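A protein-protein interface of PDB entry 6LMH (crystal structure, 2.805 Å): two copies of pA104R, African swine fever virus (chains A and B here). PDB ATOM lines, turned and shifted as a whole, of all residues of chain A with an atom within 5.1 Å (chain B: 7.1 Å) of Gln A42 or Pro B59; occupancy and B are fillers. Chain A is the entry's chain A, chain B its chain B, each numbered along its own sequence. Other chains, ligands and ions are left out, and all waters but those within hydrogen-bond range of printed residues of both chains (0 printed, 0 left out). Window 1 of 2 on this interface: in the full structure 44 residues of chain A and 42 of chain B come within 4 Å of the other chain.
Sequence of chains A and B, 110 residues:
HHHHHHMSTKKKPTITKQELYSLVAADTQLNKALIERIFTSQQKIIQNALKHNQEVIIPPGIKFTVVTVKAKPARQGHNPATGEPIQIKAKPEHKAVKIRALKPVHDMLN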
ATOM      1  N   LYS A  17      31.495 -10.017  20.315  1.00  0.00           N
ATOM      2  CA  LYS A  17      31.188  -9.699  18.925  1.00  0.00           C
ATOM      3  C   LYS A  17      31.805 -10.714  17.980  1.00  0.00           C
ATOM      4  O   LYS A  17      31.155 -11.162  17.027  1.00  0.00           O
ATOM      5  CB  LYS A  17      31.690  -8.304  18.577  1.00  0.00           C
ATOM      6  CG  LYS A  17      30.749  -7.197  18.944  1.00  0.00           C
ATOM      7  CD  LYS A  17      31.506  -5.903  19.178  1.00  0.00           C
ATOM      8  CE  LYS A  17      31.638  -5.089  17.895  1.00  0.00           C
ATOM      9  NZ  LYS A  17      31.294  -3.649  18.095  1.00  0.00           N
ATOM     10  N   LEU A  20      29.936 -13.782  18.140  1.00  0.00           N
ATOM     11  CA  LEU A  20      28.658 -13.574  17.471  1.00  0.00           C
ATOM     12  C   LEU A  20      28.798 -13.750  15.967  1.00  0.00           C
ATOM     13  O   LEU A  20      28.015 -14.477  15.345  1.00  0.00           O
ATOM     14  CB  LEU A  20      28.102 -12.189  17.797  1.00  0.00           C
ATOM     15  CG  LEU A  20      26.821 -11.840  17.041  1.00  0.00           C
ATOM     16  CD1 LEU A  20      25.602 -12.403  17.763  1.00  0.00           C
ATOM     17  CD2 LEU A  20      26.703 -10.339  16.858  1.00  0.00           C
ATOM     18  N   TYR A  21      29.796 -13.088  15.367  1.00  0.00           N
ATOM     19  CA  TYR A  21      30.069 -13.264  13.942  1.00  0.00           C
ATOM     20  C   TYR A  21      30.186 -14.741  13.585  1.00  0.00           C
ATOM     21  O   TYR A  21      29.623 -15.201  12.587  1.00  0.00           O
ATOM     22  CB  TYR A  21      31.358 -12.539  13.544  1.00  0.00           C
ATOM     23  CG  TYR A  21      31.404 -11.042  13.786  1.00  0.00           C
ATOM     24  CD1 TYR A  21      30.250 -10.267  13.771  1.00  0.00           C
ATOM     25  CD2 TYR A  21      32.624 -10.402  14.011  1.00  0.00           C
ATOM     26  CE1 TYR A  21      30.312  -8.891  13.982  1.00  0.00           C
ATOM     27  CE2 TYR A  21      32.695  -9.035  14.228  1.00  0.00           C
ATOM     28  CZ  TYR A  21      31.537  -8.283  14.211  1.00  0.00           C
ATOM     29  OH  TYR A  21      31.606  -6.923  14.424  1.00  0.00           O
ATOM     30  N   ILE A  38      28.718  -6.888   6.439  1.00  0.00           N
ATOM     31  CA  ILE A  38      27.358  -6.390   6.641  1.00  0.00           C
ATOM     32  C   ILE A  38      27.301  -5.459   7.844  1.00  0.00           C
ATOM     33  O   ILE A  38      26.793  -4.334   7.758  1.00  0.00           O
ATOM     34  CB  ILE A  38      26.370  -7.562   6.806  1.00  0.00           C
ATOM     35  CG1 ILE A  38      26.487  -8.538   5.646  1.00  0.00           C
ATOM     36  CG2 ILE A  38      24.940  -7.058   6.931  1.00  0.00           C
ATOM     37  CD1 ILE A  38      26.251  -7.902   4.315  1.00  0.00           C
ATOM     38  N   PHE A  39      27.804  -5.924   8.990  1.00  0.00           N
ATOM     39  CA  PHE A  39      27.699  -5.134  10.211  1.00  0.00           C
ATOM     40  C   PHE A  39      28.505  -3.855  10.118  1.00  0.00           C
ATOM     41  O   PHE A  39      28.118  -2.830  10.693  1.00  0.00           O
ATOM     42  CB  PHE A  39      28.146  -5.962  11.403  1.00  0.00           C
ATOM     43  CG  PHE A  39      27.241  -7.106  11.695  1.00  0.00           C
ATOM     44  CD1 PHE A  39      25.973  -6.886  12.210  1.00  0.00           C
ATOM     45  CD2 PHE A  39      27.638  -8.401  11.431  1.00  0.00           C
ATOM     46  CE1 PHE A  39      25.131  -7.944  12.477  1.00  0.00           C
ATOM     47  CE2 PHE A  39      26.796  -9.462  11.695  1.00  0.00           C
ATOM     48  CZ  PHE A  39      25.543  -9.233  12.216  1.00  0.00           C
ATOM     49  N   THR A  40      29.620  -3.890   9.392  1.00  0.00           N
ATOM     50  CA  THR A  40      30.379  -2.668   9.175  1.00  0.00           C
ATOM     51  C   THR A  40      29.590  -1.682   8.326  1.00  0.00           C
ATOM     52  O   THR A  40      29.601  -0.481   8.607  1.00  0.00           O
ATOM     53  CB  THR A  40      31.725  -2.998   8.536  1.00  0.00           C
ATOM     54  OG1 THR A  40      32.447  -3.885   9.402  1.00  0.00           O
ATOM     55  CG2 THR A  40      32.536  -1.732   8.339  1.00  0.00           C
ATOM     56  N   SER A  41      28.864  -2.168   7.311  1.00  0.00           N
ATOM     57  CA  SER A  41      28.001  -1.284   6.528  1.00  0.00           C
ATOM     58  C   SER A  41      26.898  -0.678   7.391  1.00  0.00           C
ATOM     59  O   SER A  41      26.623   0.525   7.306  1.00  0.00           O
ATOM     60  CB  SER A  41      27.389  -2.038   5.354  1.00  0.00           C
ATOM     61  OG  SER A  41      26.562  -1.170   4.593  1.00  0.00           O
ATOM     62  N   GLN A  42      26.238  -1.506   8.208  1.00  0.00           N
ATOM     63  CA  GLN A  42      25.276  -0.994   9.177  1.00  0.00           C
ATOM     64  C   GLN A  42      25.920   0.049  10.079  1.00  0.00           C
ATOM     65  O   GLN A  42      25.400   1.162  10.237  1.00  0.00           O
ATOM     66  CB  GLN A  42      24.712  -2.153  10.002  1.00  0.00           C
ATOM     67  CG  GLN A  42      23.718  -1.763  11.099  1.00  0.00           C
ATOM     68  CD  GLN A  42      23.412  -2.927  12.041  1.00  0.00           C
ATOM     69  OE1 GLN A  42      22.249  -3.244  12.295  1.00  0.00           O
ATOM     70  NE2 GLN A  42      24.460  -3.576  12.554  1.00  0.00           N
ATOM     71  N   GLN A  43      27.075  -0.294  10.658  1.00  0.00           N
ATOM     72  CA  GLN A  43      27.766   0.595  11.587  1.00  0.00           C
ATOM     73  C   GLN A  43      27.988   1.976  10.989  1.00  0.00           C
ATOM     74  O   GLN A  43      27.805   2.990  11.670  1.00  0.00           O
ATOM     75  CB  GLN A  43      29.098  -0.035  11.994  1.00  0.00           C
ATOM     76  CG  GLN A  43      29.707   0.523  13.260  1.00  0.00           C
ATOM     77  CD  GLN A  43      30.965   1.313  12.996  1.00  0.00           C
ATOM     78  OE1 GLN A  43      31.758   0.961  12.115  1.00  0.00           O
ATOM     79  NE2 GLN A  43      31.161   2.393  13.754  1.00  0.00           N
ATOM     80  N   LYS A  44      28.370   2.040   9.711  1.00  0.00           N
ATOM     81  CA  LYS A  44      28.625   3.337   9.094  1.00  0.00           C
ATOM     82  C   LYS A  44      27.333   4.057   8.731  1.00  0.00           C
ATOM     83  O   LYS A  44      27.267   5.289   8.809  1.00  0.00           O
ATOM     84  CB  LYS A  44      29.518   3.179   7.861  1.00  0.00           C
ATOM     85  CG  LYS A  44      30.659   2.191   8.062  1.00  0.00           C
ATOM     86  CD  LYS A  44      31.731   2.290   6.992  1.00  0.00           C
ATOM     87  CE  LYS A  44      31.180   2.826   5.683  1.00  0.00           C
ATOM     88  NZ  LYS A  44      32.274   3.092   4.712  1.00  0.00           N
ATOM     89  N   ILE A  45      26.299   3.315   8.330  1.00  0.00           N
ATOM     90  CA  ILE A  45      25.012   3.941   8.038  1.00  0.00           C
ATOM     91  C   ILE A  45      24.434   4.567   9.300  1.00  0.00           C
ATOM     92  O   ILE A  45      23.983   5.720   9.292  1.00  0.00           O
ATOM     93  CB  ILE A  45      24.042   2.925   7.417  1.00  0.00           C
ATOM     94  CG1 ILE A  45      24.472   2.596   5.986  1.00  0.00           C
ATOM     95  CG2 ILE A  45      22.626   3.469   7.437  1.00  0.00           C
ATOM     96  CD1 ILE A  45      23.830   1.344   5.438  1.00  0.00           C
ATOM     97  N   ILE A  46      24.440   3.816  10.406  1.00  0.00           N
ATOM     98  CA  ILE A  46      24.026   4.382  11.687  1.00  0.00           C
ATOM     99  C   ILE A  46      24.829   5.635  11.992  1.00  0.00           C
ATOM    100  O   ILE A  46      24.287   6.651  12.447  1.00  0.00           O
ATOM    101  CB  ILE A  46      24.185   3.348  12.814  1.00  0.00           C
ATOM    102  CG1 ILE A  46      23.380   2.087  12.523  1.00  0.00           C
ATOM    103  CG2 ILE A  46      23.804   3.966  14.147  1.00  0.00           C
ATOM    104  CD1 ILE A  46      23.732   0.952  13.444  1.00  0.00           C
ATOM    105  N   GLN A  47      26.136   5.579  11.752  1.00  0.00           N
ATOM    106  CA  GLN A  47      27.001   6.703  12.081  1.00  0.00           C
ATOM    107  C   GLN A  47      26.678   7.913  11.219  1.00  0.00           C
ATOM    108  O   GLN A  47      26.536   9.031  11.725  1.00  0.00           O
ATOM    109  CB  GLN A  47      28.460   6.291  11.905  1.00  0.00           C
ATOM    110  CG  GLN A  47      29.459   7.390  12.173  1.00  0.00           C
ATOM    111  CD  GLN A  47      30.832   6.832  12.410  1.00  0.00           C
ATOM    112  OE1 GLN A  47      31.287   5.954  11.675  1.00  0.00           O
ATOM    113  NE2 GLN A  47      31.495   7.314  13.455  1.00  0.00           N
ATOM    114  N   ILE A  58      17.421  -0.186  14.334  1.00  0.00           N
ATOM    115  CA  ILE A  58      18.143  -1.348  13.826  1.00  0.00           C
ATOM    116  C   ILE A  58      17.543  -2.585  14.483  1.00  0.00           C
ATOM    117  O   ILE A  58      16.907  -2.498  15.545  1.00  0.00           O
ATOM    118  CB  ILE A  58      19.660  -1.248  14.102  1.00  0.00           C
ATOM    119  CG1 ILE A  58      19.921  -1.336  15.607  1.00  0.00           C
ATOM    120  CG2 ILE A  58      20.231   0.026  13.508  1.00  0.00           C
ATOM    121  CD1 ILE A  58      21.311  -1.776  15.968  1.00  0.00           C
ATOM    122  N   PRO A  59      17.724  -3.754  13.876  1.00  0.00           N
ATOM    123  CA  PRO A  59      17.390  -4.979  14.579  1.00  0.00           C
ATOM    124  C   PRO A  59      18.290  -5.126  15.803  1.00  0.00           C
ATOM    125  O   PRO A  59      19.406  -4.590  15.830  1.00  0.00           O
ATOM    126  CB  PRO A  59      17.672  -6.075  13.544  1.00  0.00           C
ATOM    127  CG  PRO A  59      17.775  -5.371  12.233  1.00  0.00           C
ATOM    128  CD  PRO A  59      18.263  -4.008  12.531  1.00  0.00           C
ATOM    129  N   LEU B  20      16.764   0.558   6.737  1.00  0.00           N
ATOM    130  CA  LEU B  20      18.165   0.231   6.975  1.00  0.00           C
ATOM    131  C   LEU B  20      18.608  -0.926   6.094  1.00  0.00           C
ATOM    132  O   LEU B  20      19.697  -0.898   5.510  1.00  0.00           O
ATOM    133  CB  LEU B  20      18.376  -0.117   8.448  1.00  0.00           C
ATOM    134  CG  LEU B  20      19.769  -0.616   8.831  1.00  0.00           C
ATOM    135  CD1 LEU B  20      20.750   0.545   8.846  1.00  0.00           C
ATOM    136  CD2 LEU B  20      19.737  -1.323  10.180  1.00  0.00           C
ATOM    137  N   TYR B  21      17.767  -1.959   5.997  1.00  0.00           N
ATOM    138  CA  TYR B  21      18.074  -3.115   5.167  1.00  0.00           C
ATOM    139  C   TYR B  21      18.388  -2.700   3.740  1.00  0.00           C
ATOM    140  O   TYR B  21      19.355  -3.176   3.137  1.00  0.00           O
ATOM    141  CB  TYR B  21      16.901  -4.085   5.180  1.00  0.00           C
ATOM    142  CG  TYR B  21      16.583  -4.671   6.530  1.00  0.00           C
ATOM    143  CD1 TYR B  21      17.569  -4.841   7.492  1.00  0.00           C
ATOM    144  CD2 TYR B  21      15.297  -5.082   6.833  1.00  0.00           C
ATOM    145  CE1 TYR B  21      17.272  -5.398   8.727  1.00  0.00           C
ATOM    146  CE2 TYR B  21      14.990  -5.636   8.057  1.00  0.00           C
ATOM    147  CZ  TYR B  21      15.977  -5.793   9.001  1.00  0.00           C
ATOM    148  OH  TYR B  21      15.659  -6.347  10.220  1.00  0.00           O
ATOM    149  N   VAL B  24      21.844  -1.014   3.611  1.00  0.00           N
ATOM    150  CA  VAL B  24      22.901  -2.014   3.735  1.00  0.00           C
ATOM    151  C   VAL B  24      22.995  -2.846   2.462  1.00  0.00           C
ATOM    152  O   VAL B  24      24.094  -3.139   1.975  1.00  0.00           O
ATOM    153  CB  VAL B  24      22.663  -2.900   4.972  1.00  0.00           C
ATOM    154  CG1 VAL B  24      23.650  -4.056   4.992  1.00  0.00           C
ATOM    155  CG2 VAL B  24      22.774  -2.080   6.245  1.00  0.00           C
ATOM    156  N   ASP B  27      24.868  -0.638  -0.087  1.00  0.00           N
ATOM    157  CA  ASP B  27      26.279  -0.413   0.213  1.00  0.00           C
ATOM    158  C   ASP B  27      27.087  -1.688   0.023  1.00  0.00           C
ATOM    159  O   ASP B  27      28.221  -1.647  -0.469  1.00  0.00           O
ATOM    160  CB  ASP B  27      26.442   0.117   1.639  1.00  0.00           C
ATOM    161  CG  ASP B  27      27.818   0.710   1.888  1.00  0.00           C
ATOM    162  OD1 ASP B  27      28.423   1.256   0.941  1.00  0.00           O
ATOM    163  OD2 ASP B  27      28.297   0.633   3.036  1.00  0.00           O
ATOM    164  N   THR B  28      26.514  -2.833   0.393  1.00  0.00           N
ATOM    165  CA  THR B  28      27.209  -4.108   0.294  1.00  0.00           C
ATOM    166  C   THR B  28      27.042  -4.777  -1.063  1.00  0.00           C
ATOM    167  O   THR B  28      27.780  -5.720  -1.360  1.00  0.00           O
ATOM    168  CB  THR B  28      26.720  -5.065   1.386  1.00  0.00           C
ATOM    169  OG1 THR B  28      25.321  -5.326   1.204  1.00  0.00           O
ATOM    170  CG2 THR B  28      26.943  -4.469   2.758  1.00  0.00           C
ATOM    171  N   PHE B  39      20.350 -10.628   9.899  1.00  0.00           N
ATOM    172  CA  PHE B  39      19.831 -10.030  11.125  1.00  0.00           C
ATOM    173  C   PHE B  39      18.797 -10.922  11.793  1.00  0.00           C
ATOM    174  O   PHE B  39      18.712 -10.955  13.027  1.00  0.00           O
ATOM    175  CB  PHE B  39      19.246  -8.655  10.833  1.00  0.00           C
ATOM    176  CG  PHE B  39      20.287  -7.626  10.509  1.00  0.00           C
ATOM    177  CD1 PHE B  39      21.144  -7.154  11.493  1.00  0.00           C
ATOM    178  CD2 PHE B  39      20.426  -7.144   9.218  1.00  0.00           C
ATOM    179  CE1 PHE B  39      22.104  -6.208  11.198  1.00  0.00           C
ATOM    180  CE2 PHE B  39      21.391  -6.200   8.917  1.00  0.00           C
ATOM    181  CZ  PHE B  39      22.227  -5.730   9.909  1.00  0.00           C
ATOM    182  N   GLN B  42      20.828 -13.144  13.757  1.00  0.00           N
ATOM    183  CA  GLN B  42      21.363 -12.436  14.910  1.00  0.00           C
ATOM    184  C   GLN B  42      20.313 -12.300  16.005  1.00  0.00           C
ATOM    185  O   GLN B  42      20.618 -12.474  17.192  1.00  0.00           O
ATOM    186  CB  GLN B  42      21.886 -11.069  14.478  1.00  0.00           C
ATOM    187  CG  GLN B  42      22.357 -10.192  15.622  1.00  0.00           C
ATOM    188  CD  GLN B  42      22.555  -8.755  15.190  1.00  0.00           C
ATOM    189  OE1 GLN B  42      23.666  -8.233  15.241  1.00  0.00           O
ATOM    190  NE2 GLN B  42      21.475  -8.107  14.754  1.00  0.00           N
ATOM    191  N   ILE B  57      27.179  -9.372  23.136  1.00  0.00           N
ATOM    192  CA  ILE B  57      27.582  -8.071  22.610  1.00  0.00           C
ATOM    193  C   ILE B  57      27.391  -8.082  21.100  1.00  0.00           C
ATOM    194  O   ILE B  57      27.817  -9.023  20.418  1.00  0.00           O
ATOM    195  CB  ILE B  57      29.038  -7.745  22.985  1.00  0.00           C
ATOM    196  CG1 ILE B  57      29.257  -7.969  24.482  1.00  0.00           C
ATOM    197  CG2 ILE B  57      29.381  -6.320  22.614  1.00  0.00           C
ATOM    198  CD1 ILE B  57      30.596  -7.496  24.984  1.00  0.00           C
ATOM    199  N   ILE B  58      26.740  -7.051  20.575  1.00  0.00           N
ATOM    200  CA  ILE B  58      26.447  -7.014  19.144  1.00  0.00           C
ATOM    201  C   ILE B  58      27.015  -5.722  18.561  1.00  0.00           C
ATOM    202  O   ILE B  58      27.121  -4.719  19.272  1.00  0.00           O
ATOM    203  CB  ILE B  58      24.935  -7.127  18.859  1.00  0.00           C
ATOM    204  CG1 ILE B  58      24.195  -5.897  19.376  1.00  0.00           C
ATOM    205  CG2 ILE B  58      24.342  -8.418  19.444  1.00  0.00           C
ATOM    206  CD1 ILE B  58      22.906  -5.652  18.682  1.00  0.00           C
ATOM    207  N   PRO B  59      27.404  -5.711  17.279  1.00  0.00           N
ATOM    208  CA  PRO B  59      27.797  -4.434  16.683  1.00  0.00           C
ATOM    209  C   PRO B  59      26.602  -3.521  16.567  1.00  0.00           C
ATOM    210  O   PRO B  59      25.460  -3.973  16.397  1.00  0.00           O
ATOM    211  CB  PRO B  59      28.315  -4.867  15.286  1.00  0.00           C
ATOM    212  CG  PRO B  59      28.450  -6.348  15.339  1.00  0.00           C
ATOM    213  CD  PRO B  59      27.454  -6.821  16.329  1.00  0.00           C
ATOM    214  N   PRO B  60      26.814  -2.202  16.656  1.00  0.00           N
ATOM    215  CA  PRO B  60      28.118  -1.552  16.802  1.00  0.00           C
ATOM    216  C   PRO B  60      28.518  -1.256  18.242  1.00  0.00           C
ATOM    217  O   PRO B  60      28.973  -0.144  18.498  1.00  0.00           O
ATOM    218  CB  PRO B  60      27.932  -0.240  16.044  1.00  0.00           C
ATOM    219  CG  PRO B  60      26.453   0.062  16.152  1.00  0.00           C
ATOM    220  CD  PRO B  60      25.727  -1.224  16.477  1.00  0.00           C
ATOM    221  N   GLY B  61      28.398  -2.220  19.154  1.00  0.00           N
ATOM    222  CA  GLY B  61      28.767  -1.949  20.531  1.00  0.00           C
ATOM    223  C   GLY B  61      27.630  -1.723  21.506  1.00  0.00           C
ATOM    224  O   GLY B  61      27.576  -0.686  22.177  1.00  0.00           O
ATOM    225  N   ILE B  62      26.685  -2.659  21.552  1.00  0.00           N
ATOM    226  CA  ILE B  62      25.596  -2.659  22.522  1.00  0.00           C
ATOM    227  C   ILE B  62      25.647  -3.971  23.293  1.00  0.00           C
ATOM    228  O   ILE B  62      25.775  -5.042  22.686  1.00  0.00           O
ATOM    229  CB  ILE B  62      24.234  -2.471  21.829  1.00  0.00           C
ATOM    230  CG1 ILE B  62      24.174  -1.083  21.187  1.00  0.00           C
ATOM    231  CG2 ILE B  62      23.102  -2.643  22.819  1.00  0.00           C
ATOM    232  CD1 ILE B  62      23.083  -0.925  20.155  1.00  0.00           C
ATOM    233  N   PHE B  64      23.828  -6.707  25.870  1.00  0.00           N
ATOM    234  CA  PHE B  64      22.521  -7.211  26.276  1.00  0.00           C
ATOM    235  C   PHE B  64      22.645  -7.944  27.601  1.00  0.00           C
ATOM    236  O   PHE B  64      23.435  -8.886  27.722  1.00  0.00           O
ATOM    237  CB  PHE B  64      21.935  -8.154  25.221  1.00  0.00           C
ATOM    238  CG  PHE B  64      21.378  -7.446  24.018  1.00  0.00           C
ATOM    239  CD1 PHE B  64      22.224  -6.941  23.046  1.00  0.00           C
ATOM    240  CD2 PHE B  64      20.013  -7.279  23.864  1.00  0.00           C
ATOM    241  CE1 PHE B  64      21.721  -6.287  21.945  1.00  0.00           C
ATOM    242  CE2 PHE B  64      19.501  -6.618  22.769  1.00  0.00           C
ATOM    243  CZ  PHE B  64      20.356  -6.122  21.805  1.00  0.00           C
ATOM    244  N   VAL B 105      29.531   3.332  20.392  1.00  0.00           N
ATOM    245  CA  VAL B 105      28.265   4.025  20.192  1.00  0.00           C
ATOM    246  C   VAL B 105      28.321   5.410  20.822  1.00  0.00           C
ATOM    247  O   VAL B 105      27.950   6.408  20.194  1.00  0.00           O
ATOM    248  CB  VAL B 105      27.102   3.178  20.737  1.00  0.00           C
ATOM    249  CG1 VAL B 105      25.783   3.947  20.693  1.00  0.00           C
ATOM    250  CG2 VAL B 105      26.980   1.895  19.927  1.00  0.00           C
ATOM    251  N   MET B 108      30.070   7.861  18.573  1.00  0.00           N
ATOM    252  CA  MET B 108      29.664   7.854  17.169  1.00  0.00           C
ATOM    253  C   MET B 108      29.631   9.250  16.561  1.00  0.00           C
ATOM    254  O   MET B 108      29.777   9.395  15.342  1.00  0.00           O
ATOM    255  CB  MET B 108      28.295   7.193  17.027  1.00  0.00           C
ATOM    256  CG  MET B 108      28.118   6.365  15.772  1.00  0.00           C
ATOM    257  SD  MET B 108      27.126   4.901  16.106  1.00  0.00           S
ATOM    258  CE  MET B 108      27.430   3.947  14.621  1.00  0.00           C
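Tyr A21 touches Pro B59, and with the chains exchanged Pro A59 touches Tyr B21.
Phe A39 touches Pro B59, and with the chains exchanged Pro A59 touches Phe B39.
Gln A42 touches Leu B20, but with the chains exchanged Leu A20 does not touch Gln B42 (4.03 Å).
Gln A42 touches Pro B59, but with the chains exchanged Pro A59 does not touch Gln B42 (4.2 Å).
6 positions are printed for both chains.
Printed residues of chain A that touch a printed residue of chain B: Lys A17, Leu A20, Tyr A21, Ile A38, Phe A39, Ser A41, Gln A42, Gln A43, Ile A45, Ile A46, Gln A47, Ile A58 and Pro A59.
Hydrophobic or aromatic side chains of chain A within 4 Å of the printed part of chain B: Leu A20, Tyr A21, Ile A38, Phe A39, Ile A45, Ile A46, Ile A58 and Pro A59.
Along chain A the printed residues that touch a printed residue of chain B span positions 17 to 59.
Printed residues of chain B that touch a printed residue of chain A: Leu B20, Tyr B21, Val B24, Asp B27, Thr B28, Phe B39, Gln B42, Ile B57, Ile B58, Pro B59, Pro B60, Gly B61 and Met B108.
Hydrophobic or aromatic side chains of chain B that line the printed part of chain A: Leu B20, Tyr B21, Val B24, Phe B39, Ile B58, Pro B59, Pro B60 and Met B108.
Printed residues of chain A within 4 Å of Pro B59: Lys A17 (3.9 Å), Leu A20 (3.6 Å), Tyr A21 (3.3 Å), Phe A39 (3.9 Å) and Gln A42 (3.99 Å).
Printed residues of chain A within 4 Å of Pro B60: Lys A17, Gln A43 and Ile A46.
Printed residues of chain B within 4 Å of Pro A59: Leu B20 (3.9 Å), Tyr B21 (3.1 Å) and Phe B39 (3.8 Å).
Of the printed residues of chain B, Gln A43 touches Pro B60 and Met B108.
Of the printed residues of chain A, Asp B27 touches Ser A41.
Printed residues of chain B within 4 Å of Lys A17: Ile B57 (3.7 Å), Pro B59 (3.9 Å), Pro B60 (3.7 Å) and Gly B61 (3.4 Å).
Phe B64 touches none of the printed residues of chain A.
Ile B62 touches none of the printed residues of chain A.
The nearest printed residue of chain B that does not touch Pro A59 is Gln B42 (4.2 Å).
The side-chain hydroxyl (OG1) of Thr B28 is in hydrogen-bond range of the backbone carbonyl oxygen (O) of Val B24 (2.6 Å).
OD2 of Asp B27 is in hydrogen-bond range of OG of Ser A41 (2.9 Å).
The side-chain amide nitrogen (NE2) of Gln A47 lies within hydrogen-bond range of the backbone carbonyl oxygen (O) of Met B108 (3.3 Å).
The side-chain amino group (NZ) of Lys A17 lies close to the backbone NH (N) of Gly B61 (3.4 Å).
NZ of Lys A17 touches CA of Pro B59 (3.9 Å).
CD of Pro B59 touches CD2 of Leu A20, at 3.6 Å.
Tyr A21 touches Pro B59.
Gln A42 touches Leu B20.
Gln A43 touches Pro B60 (CG to CB, 3.4 Å).
O of Gln A43 touches CE of Met B108 (3.1 Å).
N of Val B24 touches CD1 of Ile A45 (3.6 Å).
Ile A46 touches Met B108.
Leu B20 touches Ile A58.
Pro A59 touches Leu B20.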
